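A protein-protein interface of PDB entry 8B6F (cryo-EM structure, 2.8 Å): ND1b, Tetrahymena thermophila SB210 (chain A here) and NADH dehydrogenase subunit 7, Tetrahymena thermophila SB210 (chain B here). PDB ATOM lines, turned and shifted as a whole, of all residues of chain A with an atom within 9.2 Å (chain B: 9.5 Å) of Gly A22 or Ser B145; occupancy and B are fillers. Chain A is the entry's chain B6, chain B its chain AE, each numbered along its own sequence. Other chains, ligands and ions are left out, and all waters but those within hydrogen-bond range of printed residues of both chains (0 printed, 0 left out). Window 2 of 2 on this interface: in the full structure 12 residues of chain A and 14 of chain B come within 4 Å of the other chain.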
ATOM      1  N   CYS A  14      14.209  20.776   2.030  1.00  0.00           N
ATOM      2  CA  CYS A  14      14.112  19.663   2.968  1.00  0.00           C
ATOM      3  C   CYS A  14      12.789  19.701   3.721  1.00  0.00           C
ATOM      4  O   CYS A  14      12.148  18.662   3.917  1.00  0.00           O
ATOM      5  CB  CYS A  14      15.287  19.694   3.944  1.00  0.00           C
ATOM      6  SG  CYS A  14      16.857  19.183   3.216  1.00  0.00           S
ATOM      7  N   VAL A  15      12.366  20.888   4.156  1.00  0.00           N
ATOM      8  CA  VAL A  15      11.077  21.012   4.829  1.00  0.00           C
ATOM      9  C   VAL A  15       9.948  20.635   3.879  1.00  0.00           C
ATOM     10  O   VAL A  15       8.973  19.987   4.277  1.00  0.00           O
ATOM     11  CB  VAL A  15      10.902  22.436   5.391  1.00  0.00           C
ATOM     12  CG1 VAL A  15       9.486  22.648   5.918  1.00  0.00           C
ATOM     13  CG2 VAL A  15      11.918  22.696   6.489  1.00  0.00           C
ATOM     14  N   VAL A  16      10.056  21.039   2.612  1.00  0.00           N
ATOM     15  CA  VAL A  16       9.038  20.671   1.631  1.00  0.00           C
ATOM     16  C   VAL A  16       8.960  19.156   1.490  1.00  0.00           C
ATOM     17  O   VAL A  16       7.868  18.577   1.454  1.00  0.00           O
ATOM     18  CB  VAL A  16       9.326  21.357   0.282  1.00  0.00           C
ATOM     19  CG1 VAL A  16       8.492  20.744  -0.836  1.00  0.00           C
ATOM     20  CG2 VAL A  16       9.059  22.851   0.377  1.00  0.00           C
ATOM     21  N   ALA A  17      10.113  18.492   1.401  1.00  0.00           N
ATOM     22  CA  ALA A  17      10.116  17.038   1.270  1.00  0.00           C
ATOM     23  C   ALA A  17       9.506  16.371   2.495  1.00  0.00           C
ATOM     24  O   ALA A  17       8.743  15.407   2.374  1.00  0.00           O
ATOM     25  CB  ALA A  17      11.541  16.535   1.049  1.00  0.00           C
ATOM     26  N   ILE A  18       9.845  16.863   3.687  1.00  0.00           N
ATOM     27  CA  ILE A  18       9.310  16.286   4.916  1.00  0.00           C
ATOM     28  C   ILE A  18       7.798  16.449   4.957  1.00  0.00           C
ATOM     29  O   ILE A  18       7.061  15.515   5.293  1.00  0.00           O
ATOM     30  CB  ILE A  18       9.980  16.944   6.134  1.00  0.00           C
ATOM     31  CG1 ILE A  18      11.477  16.630   6.137  1.00  0.00           C
ATOM     32  CG2 ILE A  18       9.335  16.453   7.423  1.00  0.00           C
ATOM     33  CD1 ILE A  18      12.306  17.655   6.873  1.00  0.00           C
ATOM     34  N   ALA A  19       7.313  17.644   4.622  1.00  0.00           N
ATOM     35  CA  ALA A  19       5.875  17.875   4.616  1.00  0.00           C
ATOM     36  C   ALA A  19       5.184  16.986   3.593  1.00  0.00           C
ATOM     37  O   ALA A  19       4.151  16.379   3.886  1.00  0.00           O
ATOM     38  CB  ALA A  19       5.581  19.348   4.338  1.00  0.00           C
ATOM     39  N   THR A  20       5.788  16.824   2.417  1.00  0.00           N
ATOM     40  CA  THR A  20       5.206  15.959   1.398  1.00  0.00           C
ATOM     41  C   THR A  20       5.133  14.517   1.876  1.00  0.00           C
ATOM     42  O   THR A  20       4.133  13.828   1.643  1.00  0.00           O
ATOM     43  CB  THR A  20       6.012  16.055   0.105  1.00  0.00           C
ATOM     44  OG1 THR A  20       6.049  17.417  -0.335  1.00  0.00           O
ATOM     45  CG2 THR A  20       5.376  15.206  -0.976  1.00  0.00           C
ATOM     46  N   ARG A  21       6.179  14.039   2.545  1.00  0.00           N
ATOM     47  CA  ARG A  21       6.138  12.687   3.087  1.00  0.00           C
ATOM     48  C   ARG A  21       5.017  12.549   4.109  1.00  0.00           C
ATOM     49  O   ARG A  21       4.333  11.521   4.155  1.00  0.00           O
ATOM     50  CB  ARG A  21       7.487  12.329   3.706  1.00  0.00           C
ATOM     51  CG  ARG A  21       7.585  10.888   4.174  1.00  0.00           C
ATOM     52  CD  ARG A  21       7.246  10.742   5.646  1.00  0.00           C
ATOM     53  NE  ARG A  21       8.363  11.129   6.498  1.00  0.00           N
ATOM     54  CZ  ARG A  21       9.300  10.299   6.937  1.00  0.00           C
ATOM     55  NH1 ARG A  21       9.290   9.014   6.623  1.00  0.00           N
ATOM     56  NH2 ARG A  21      10.273  10.771   7.711  1.00  0.00           N
ATOM     57  N   GLY A  22       4.819  13.570   4.942  1.00  0.00           N
ATOM     58  CA  GLY A  22       3.749  13.530   5.922  1.00  0.00           C
ATOM     59  C   GLY A  22       2.357  13.650   5.332  1.00  0.00           C
ATOM     60  O   GLY A  22       1.392  13.214   5.967  1.00  0.00           O
ATOM     61  N   THR A  23       2.225  14.237   4.141  1.00  0.00           N
ATOM     62  CA  THR A  23       0.908  14.471   3.551  1.00  0.00           C
ATOM     63  C   THR A  23       0.485  13.349   2.604  1.00  0.00           C
ATOM     64  O   THR A  23      -0.548  12.708   2.816  1.00  0.00           O
ATOM     65  CB  THR A  23       0.885  15.807   2.790  1.00  0.00           C
ATOM     66  OG1 THR A  23       1.780  15.747   1.673  1.00  0.00           O
ATOM     67  CG2 THR A  23       1.254  16.966   3.689  1.00  0.00           C
ATOM     68  N   LEU A  24       1.269  13.108   1.559  1.00  0.00           N
ATOM     69  CA  LEU A  24       0.800  12.322   0.429  1.00  0.00           C
ATOM     70  C   LEU A  24       0.786  10.825   0.726  1.00  0.00           C
ATOM     71  O   LEU A  24       1.501  10.346   1.611  1.00  0.00           O
ATOM     72  CB  LEU A  24       1.672  12.587  -0.793  1.00  0.00           C
ATOM     73  CG  LEU A  24       1.512  13.953  -1.463  1.00  0.00           C
ATOM     74  CD1 LEU A  24       2.475  14.076  -2.621  1.00  0.00           C
ATOM     75  CD2 LEU A  24       0.087  14.185  -1.940  1.00  0.00           C
ATOM     76  N   PRO A  25      -0.033  10.056  -0.010  1.00  0.00           N
ATOM     77  CA  PRO A  25       0.028   8.590   0.090  1.00  0.00           C
ATOM     78  C   PRO A  25       1.226   8.022  -0.651  1.00  0.00           C
ATOM     79  O   PRO A  25       2.089   8.777  -1.106  1.00  0.00           O
ATOM     80  CB  PRO A  25      -1.292   8.128  -0.550  1.00  0.00           C
ATOM     81  CG  PRO A  25      -2.106   9.364  -0.760  1.00  0.00           C
ATOM     82  CD  PRO A  25      -1.139  10.489  -0.878  1.00  0.00           C
ATOM     83  N   VAL B 134     -10.825   4.240   8.831  1.00  0.00           N
ATOM     84  CA  VAL B 134     -10.309   5.117   7.786  1.00  0.00           C
ATOM     85  C   VAL B 134      -8.864   5.498   8.078  1.00  0.00           C
ATOM     86  O   VAL B 134      -8.032   5.576   7.167  1.00  0.00           O
ATOM     87  CB  VAL B 134     -11.207   6.359   7.640  1.00  0.00           C
ATOM     88  CG1 VAL B 134     -10.601   7.352   6.657  1.00  0.00           C
ATOM     89  CG2 VAL B 134     -12.598   5.955   7.187  1.00  0.00           C
ATOM     90  N   ALA B 135      -8.544   5.748   9.348  1.00  0.00           N
ATOM     91  CA  ALA B 135      -7.171   6.082   9.706  1.00  0.00           C
ATOM     92  C   ALA B 135      -6.219   4.936   9.394  1.00  0.00           C
ATOM     93  O   ALA B 135      -5.134   5.152   8.843  1.00  0.00           O
ATOM     94  CB  ALA B 135      -7.098   6.443  11.188  1.00  0.00           C
ATOM     95  N   CYS B 136      -6.605   3.708   9.743  1.00  0.00           N
ATOM     96  CA  CYS B 136      -5.749   2.562   9.461  1.00  0.00           C
ATOM     97  C   CYS B 136      -5.629   2.322   7.962  1.00  0.00           C
ATOM     98  O   CYS B 136      -4.553   1.973   7.467  1.00  0.00           O
ATOM     99  CB  CYS B 136      -6.289   1.318  10.163  1.00  0.00           C
ATOM    100  SG  CYS B 136      -6.146   1.371  11.965  1.00  0.00           S
ATOM    101  N   ALA B 138      -5.798   4.630   5.608  1.00  0.00           N
ATOM    102  CA  ALA B 138      -4.891   5.653   5.099  1.00  0.00           C
ATOM    103  C   ALA B 138      -3.447   5.347   5.477  1.00  0.00           C
ATOM    104  O   ALA B 138      -2.530   5.554   4.676  1.00  0.00           O
ATOM    105  CB  ALA B 138      -5.303   7.027   5.626  1.00  0.00           C
ATOM    106  N   LEU B 139      -3.227   4.854   6.698  1.00  0.00           N
ATOM    107  CA  LEU B 139      -1.878   4.496   7.118  1.00  0.00           C
ATOM    108  C   LEU B 139      -1.314   3.372   6.260  1.00  0.00           C
ATOM    109  O   LEU B 139      -0.146   3.411   5.860  1.00  0.00           O
ATOM    110  CB  LEU B 139      -1.880   4.096   8.594  1.00  0.00           C
ATOM    111  CG  LEU B 139      -0.509   3.895   9.244  1.00  0.00           C
ATOM    112  CD1 LEU B 139       0.279   5.195   9.275  1.00  0.00           C
ATOM    113  CD2 LEU B 139      -0.663   3.334  10.646  1.00  0.00           C
ATOM    114  N   GLY B 142      -0.411   4.729   2.887  1.00  0.00           N
ATOM    115  CA  GLY B 142       0.796   5.528   2.964  1.00  0.00           C
ATOM    116  C   GLY B 142       0.638   6.842   3.699  1.00  0.00           C
ATOM    117  O   GLY B 142       1.608   7.354   4.262  1.00  0.00           O
ATOM    118  N   SER B 143      -0.570   7.398   3.711  1.00  0.00           N
ATOM    119  CA  SER B 143      -0.788   8.666   4.392  1.00  0.00           C
ATOM    120  C   SER B 143      -0.607   8.490   5.895  1.00  0.00           C
ATOM    121  O   SER B 143      -1.111   7.537   6.491  1.00  0.00           O
ATOM    122  CB  SER B 143      -2.187   9.198   4.081  1.00  0.00           C
ATOM    123  OG  SER B 143      -2.400  10.464   4.681  1.00  0.00           O
ATOM    124  N   MET B 144       0.109   9.432   6.509  1.00  0.00           N
ATOM    125  CA  MET B 144       0.560   9.297   7.891  1.00  0.00           C
ATOM    126  C   MET B 144      -0.300  10.086   8.871  1.00  0.00           C
ATOM    127  O   MET B 144      -0.863   9.512   9.804  1.00  0.00           O
ATOM    128  CB  MET B 144       2.024   9.743   7.999  1.00  0.00           C
ATOM    129  CG  MET B 144       2.648   9.493   9.367  1.00  0.00           C
ATOM    130  SD  MET B 144       4.316  10.163   9.510  1.00  0.00           S
ATOM    131  CE  MET B 144       5.167   9.234   8.240  1.00  0.00           C
ATOM    132  N   SER B 145      -0.421  11.398   8.671  1.00  0.00           N
ATOM    133  CA  SER B 145      -1.006  12.261   9.690  1.00  0.00           C
ATOM    134  C   SER B 145      -2.488  11.997   9.915  1.00  0.00           C
ATOM    135  O   SER B 145      -3.026  12.422  10.942  1.00  0.00           O
ATOM    136  CB  SER B 145      -0.799  13.724   9.311  1.00  0.00           C
ATOM    137  OG  SER B 145       0.581  14.000   9.149  1.00  0.00           O
ATOM    138  N   SER B 146      -3.156  11.305   8.995  1.00  0.00           N
ATOM    139  CA  SER B 146      -4.568  11.002   9.193  1.00  0.00           C
ATOM    140  C   SER B 146      -4.797  10.205  10.470  1.00  0.00           C
ATOM    141  O   SER B 146      -5.833  10.367  11.123  1.00  0.00           O
ATOM    142  CB  SER B 146      -5.117  10.240   7.988  1.00  0.00           C
ATOM    143  OG  SER B 146      -5.091  11.045   6.822  1.00  0.00           O
ATOM    144  N   VAL B 147      -3.850   9.344  10.845  1.00  0.00           N
ATOM    145  CA  VAL B 147      -4.020   8.556  12.062  1.00  0.00           C
ATOM    146  C   VAL B 147      -4.057   9.469  13.280  1.00  0.00           C
ATOM    147  O   VAL B 147      -4.897   9.302  14.172  1.00  0.00           O
ATOM    148  CB  VAL B 147      -2.919   7.482  12.177  1.00  0.00           C
ATOM    149  CG1 VAL B 147      -1.561   8.090  12.500  1.00  0.00           C
ATOM    150  CG2 VAL B 147      -3.298   6.445  13.219  1.00  0.00           C
ATOM    151  N   PHE B 148      -3.149  10.445  13.346  1.00  0.00           N
ATOM    152  CA  PHE B 148      -3.173  11.377  14.468  1.00  0.00           C
ATOM    153  C   PHE B 148      -4.464  12.188  14.481  1.00  0.00           C
ATOM    154  O   PHE B 148      -5.073  12.379  15.538  1.00  0.00           O
ATOM    155  CB  PHE B 148      -1.963  12.310  14.395  1.00  0.00           C
ATOM    156  CG  PHE B 148      -0.645  11.607  14.544  1.00  0.00           C
ATOM    157  CD1 PHE B 148      -0.099  10.900  13.487  1.00  0.00           C
ATOM    158  CD2 PHE B 148       0.061  11.675  15.732  1.00  0.00           C
ATOM    159  CE1 PHE B 148       1.114  10.257  13.617  1.00  0.00           C
ATOM    160  CE2 PHE B 148       1.277  11.035  15.868  1.00  0.00           C
ATOM    161  CZ  PHE B 148       1.804  10.326  14.810  1.00  0.00           C
ATOM    162  N   TRP B 149      -4.886  12.687  13.317  1.00  0.00           N
ATOM    163  CA  TRP B 149      -6.085  13.515  13.260  1.00  0.00           C
ATOM    164  C   TRP B 149      -7.319  12.740  13.700  1.00  0.00           C
ATOM    165  O   TRP B 149      -8.162  13.263  14.437  1.00  0.00           O
ATOM    166  CB  TRP B 149      -6.276  14.062  11.848  1.00  0.00           C
ATOM    167  CG  TRP B 149      -5.124  14.883  11.382  1.00  0.00           C
ATOM    168  CD1 TRP B 149      -4.249  15.583  12.158  1.00  0.00           C
ATOM    169  CD2 TRP B 149      -4.707  15.081  10.029  1.00  0.00           C
ATOM    170  NE1 TRP B 149      -3.316  16.209  11.372  1.00  0.00           N
ATOM    171  CE2 TRP B 149      -3.575  15.918  10.059  1.00  0.00           C
ATOM    172  CE3 TRP B 149      -5.183  14.633   8.793  1.00  0.00           C
ATOM    173  CZ2 TRP B 149      -2.911  16.315   8.904  1.00  0.00           C
ATOM    174  CZ3 TRP B 149      -4.524  15.029   7.646  1.00  0.00           C
ATOM    175  CH2 TRP B 149      -3.399  15.863   7.708  1.00  0.00           C
ATOM    176  N   ALA B 150      -7.441  11.488  13.258  1.00  0.00           N
ATOM    177  CA  ALA B 150      -8.583  10.673  13.651  1.00  0.00           C
ATOM    178  C   ALA B 150      -8.506  10.276  15.116  1.00  0.00           C
ATOM    179  O   ALA B 150      -9.526  10.250  15.812  1.00  0.00           O
ATOM    180  CB  ALA B 150      -8.664   9.427  12.770  1.00  0.00           C
ATOM    181  N   PHE B 151      -7.305   9.973  15.606  1.00  0.00           N
ATOM    182  CA  PHE B 151      -7.173   9.500  16.975  1.00  0.00           C
ATOM    183  C   PHE B 151      -7.387  10.604  17.999  1.00  0.00           C
ATOM    184  O   PHE B 151      -7.720  10.300  19.145  1.00  0.00           O
ATOM    185  CB  PHE B 151      -5.811   8.843  17.174  1.00  0.00           C
ATOM    186  CG  PHE B 151      -5.812   7.370  16.888  1.00  0.00           C
ATOM    187  CD1 PHE B 151      -5.928   6.893  15.595  1.00  0.00           C
ATOM    188  CD2 PHE B 151      -5.702   6.462  17.922  1.00  0.00           C
ATOM    189  CE1 PHE B 151      -5.935   5.535  15.342  1.00  0.00           C
ATOM    190  CE2 PHE B 151      -5.709   5.107  17.680  1.00  0.00           C
ATOM    191  CZ  PHE B 151      -5.823   4.640  16.388  1.00  0.00           C
ATOM    192  N   GLU B 152      -7.238  11.871  17.615  1.00  0.00           N
ATOM    193  CA  GLU B 152      -7.643  12.952  18.508  1.00  0.00           C
ATOM    194  C   GLU B 152      -9.140  12.894  18.780  1.00  0.00           C
ATOM    195  O   GLU B 152      -9.578  12.967  19.933  1.00  0.00           O
ATOM    196  CB  GLU B 152      -7.253  14.305  17.914  1.00  0.00           C
ATOM    197  CG  GLU B 152      -7.657  15.496  18.774  1.00  0.00           C
ATOM    198  CD  GLU B 152      -6.981  15.498  20.133  1.00  0.00           C
ATOM    199  OE1 GLU B 152      -6.074  14.669  20.351  1.00  0.00           O
ATOM    200  OE2 GLU B 152      -7.357  16.332  20.984  1.00  0.00           O
ATOM    201  N   THR B 202     -12.444  18.051  11.551  1.00  0.00           N
ATOM    202  CA  THR B 202     -11.603  16.877  11.343  1.00  0.00           C
ATOM    203  C   THR B 202     -12.012  16.128  10.082  1.00  0.00           C
ATOM    204  O   THR B 202     -11.153  15.655   9.330  1.00  0.00           O
ATOM    205  CB  THR B 202     -11.669  15.957  12.560  1.00  0.00           C
ATOM    206  OG1 THR B 202     -11.200  16.659  13.716  1.00  0.00           O
ATOM    207  CG2 THR B 202     -10.814  14.715  12.343  1.00  0.00           C
ATOM    208  N   GLU B 205     -10.611  18.043   7.214  1.00  0.00           N
ATOM    209  CA  GLU B 205      -9.159  17.911   7.133  1.00  0.00           C
ATOM    210  C   GLU B 205      -8.768  16.597   6.467  1.00  0.00           C
ATOM    211  O   GLU B 205      -7.887  16.564   5.601  1.00  0.00           O
ATOM    212  CB  GLU B 205      -8.549  18.012   8.531  1.00  0.00           C
ATOM    213  CG  GLU B 205      -8.508  19.430   9.074  1.00  0.00           C
ATOM    214  CD  GLU B 205      -7.941  19.501  10.475  1.00  0.00           C
ATOM    215  OE1 GLU B 205      -7.839  18.443  11.129  1.00  0.00           O
ATOM    216  OE2 GLU B 205      -7.599  20.614  10.923  1.00  0.00           O
ATOM    217  N   MET B 206      -9.415  15.499   6.861  1.00  0.00           N
ATOM    218  CA  MET B 206      -9.145  14.217   6.222  1.00  0.00           C
ATOM    219  C   MET B 206      -9.629  14.221   4.777  1.00  0.00           C
ATOM    220  O   MET B 206      -8.963  13.681   3.888  1.00  0.00           O
ATOM    221  CB  MET B 206      -9.801  13.084   7.009  1.00  0.00           C
ATOM    222  CG  MET B 206      -9.323  12.982   8.450  1.00  0.00           C
ATOM    223  SD  MET B 206     -10.130  11.662   9.377  1.00  0.00           S
ATOM    224  CE  MET B 206      -9.561  10.214   8.487  1.00  0.00           C
ATOM    225  N   VAL B 209      -7.253  15.910   2.101  1.00  0.00           N
ATOM    226  CA  VAL B 209      -6.041  15.189   1.721  1.00  0.00           C
ATOM    227  C   VAL B 209      -6.298  13.806   1.129  1.00  0.00           C
ATOM    228  O   VAL B 209      -5.398  13.250   0.486  1.00  0.00           O
ATOM    229  CB  VAL B 209      -5.085  15.057   2.924  1.00  0.00           C
ATOM    230  CG1 VAL B 209      -4.718  16.429   3.463  1.00  0.00           C
ATOM    231  CG2 VAL B 209      -5.699  14.199   4.020  1.00  0.00           C
ATOM    232  N   LEU B 210      -7.488  13.238   1.314  1.00  0.00           N
ATOM    233  CA  LEU B 210      -7.780  11.896   0.821  1.00  0.00           C
ATOM    234  C   LEU B 210      -8.733  11.876  -0.366  1.00  0.00           C
ATOM    235  O   LEU B 210      -8.433  11.250  -1.385  1.00  0.00           O
ATOM    236  CB  LEU B 210      -8.373  11.052   1.961  1.00  0.00           C
ATOM    237  CG  LEU B 210      -7.459  10.751   3.153  1.00  0.00           C
ATOM    238  CD1 LEU B 210      -8.185   9.907   4.186  1.00  0.00           C
ATOM    239  CD2 LEU B 210      -6.180  10.062   2.712  1.00  0.00           C
ATOM    240  N   ASN B 213      -7.498  13.410  -3.821  1.00  0.00           N
ATOM    241  CA  ASN B 213      -6.107  13.171  -4.175  1.00  0.00           C
ATOM    242  C   ASN B 213      -6.024  12.176  -5.324  1.00  0.00           C
ATOM    243  O   ASN B 213      -6.670  11.123  -5.296  1.00  0.00           O
ATOM    244  CB  ASN B 213      -5.335  12.657  -2.963  1.00  0.00           C
ATOM    245  CG  ASN B 213      -3.840  12.810  -3.122  1.00  0.00           C
ATOM    246  OD1 ASN B 213      -3.309  12.712  -4.225  1.00  0.00           O
ATOM    247  ND2 ASN B 213      -3.151  13.058  -2.017  1.00  0.00           N
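The backbone carbonyl oxygen of Ala B138 sits at hydrogen-bond distance from the backbone NH of Ser B143 (2.9 Å).
The side-chain hydroxyl (OG) of Ser B143 lies within hydrogen-bond range of the side-chain hydroxyl (OG) of Ser B146, at 3.5 Å.
The backbone carbonyl oxygen of Val B209 lies within hydrogen-bond range of the side-chain amide nitrogen of Asn B213 (3.4 Å).
O of Ala A19 lies close to OG1 of Thr A23 (3.3 Å).
O of Thr A20 lies within hydrogen-bond range of OG1 of Thr A23, 3.0 Å away.
Arg A21 touches Met B144.
Gly B142 touches Leu A24 (O to O, 3.999 Å).
Leu A24 touches Ser B143 (O to CA, 3.97 Å).
Asn B213 touches Leu A24 (ND2 to CD2, 3.4 Å).
Pro A25 touches Ser B143 (CA to N, 3.9 Å).
Pro A25 touches Asn B213 (CD to ND2, 3.5 Å).
The backbone carbonyl oxygen (O) of Thr A23 is in hydrogen-bond range of the side-chain hydroxyl (OG) of Ser B143, at 3.5 Å.
The backbone carbonyl oxygen (O) of Gly A22 sits at hydrogen-bond distance from the side-chain hydroxyl (OG) of Ser B145, at 3.4 Å.
Of the 22 printed residues of chain B, 5 touch a printed residue of chain A.
Printed residues of chain B that touch a printed residue of chain A: Gly B142, Ser B143, Met B144, Ser B145 and Asn B213.
Hydrophobic or aromatic side chains of chain B within 4 Å of the printed part of chain A: Met B144.
Among the printed residues, 8 pairs touch across the chains.
Among the printed residues, no Asp or Glu carboxylate lies within 4 Å of a Lys or Arg side-chain nitrogen of the other chain.
Printed residues of chain B within 4 Å of Arg A21: Met B144 (3.7 Å).
Gly A22 touches just one residue of chain B: Ser B145 (3.4 Å).
Of chain B, only Ser B143 (3.5 Å) comes within 4 Å of Thr A23.
Of the printed residues of chain B, Leu A24 touches Gly B142 (3.999 Å), Ser B143 (3.97 Å) and Asn B213 (3.4 Å).
Of the printed residues of chain B, Pro A25 touches Ser B143 (3.9 Å) and Asn B213 (3.5 Å).
Printed residues of chain A within 4 Å of Ser B143: Thr A23 (3.5 Å), Leu A24 (3.97 Å) and Pro A25 (3.9 Å).
Of chain A, only Arg A21 (3.7 Å) comes within 4 Å of Met B144.
Ser B146 touches none of the printed residues of chain A.
The nearest residue of chain A that does not touch Ser B145 is Thr A23 (5.3 Å).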
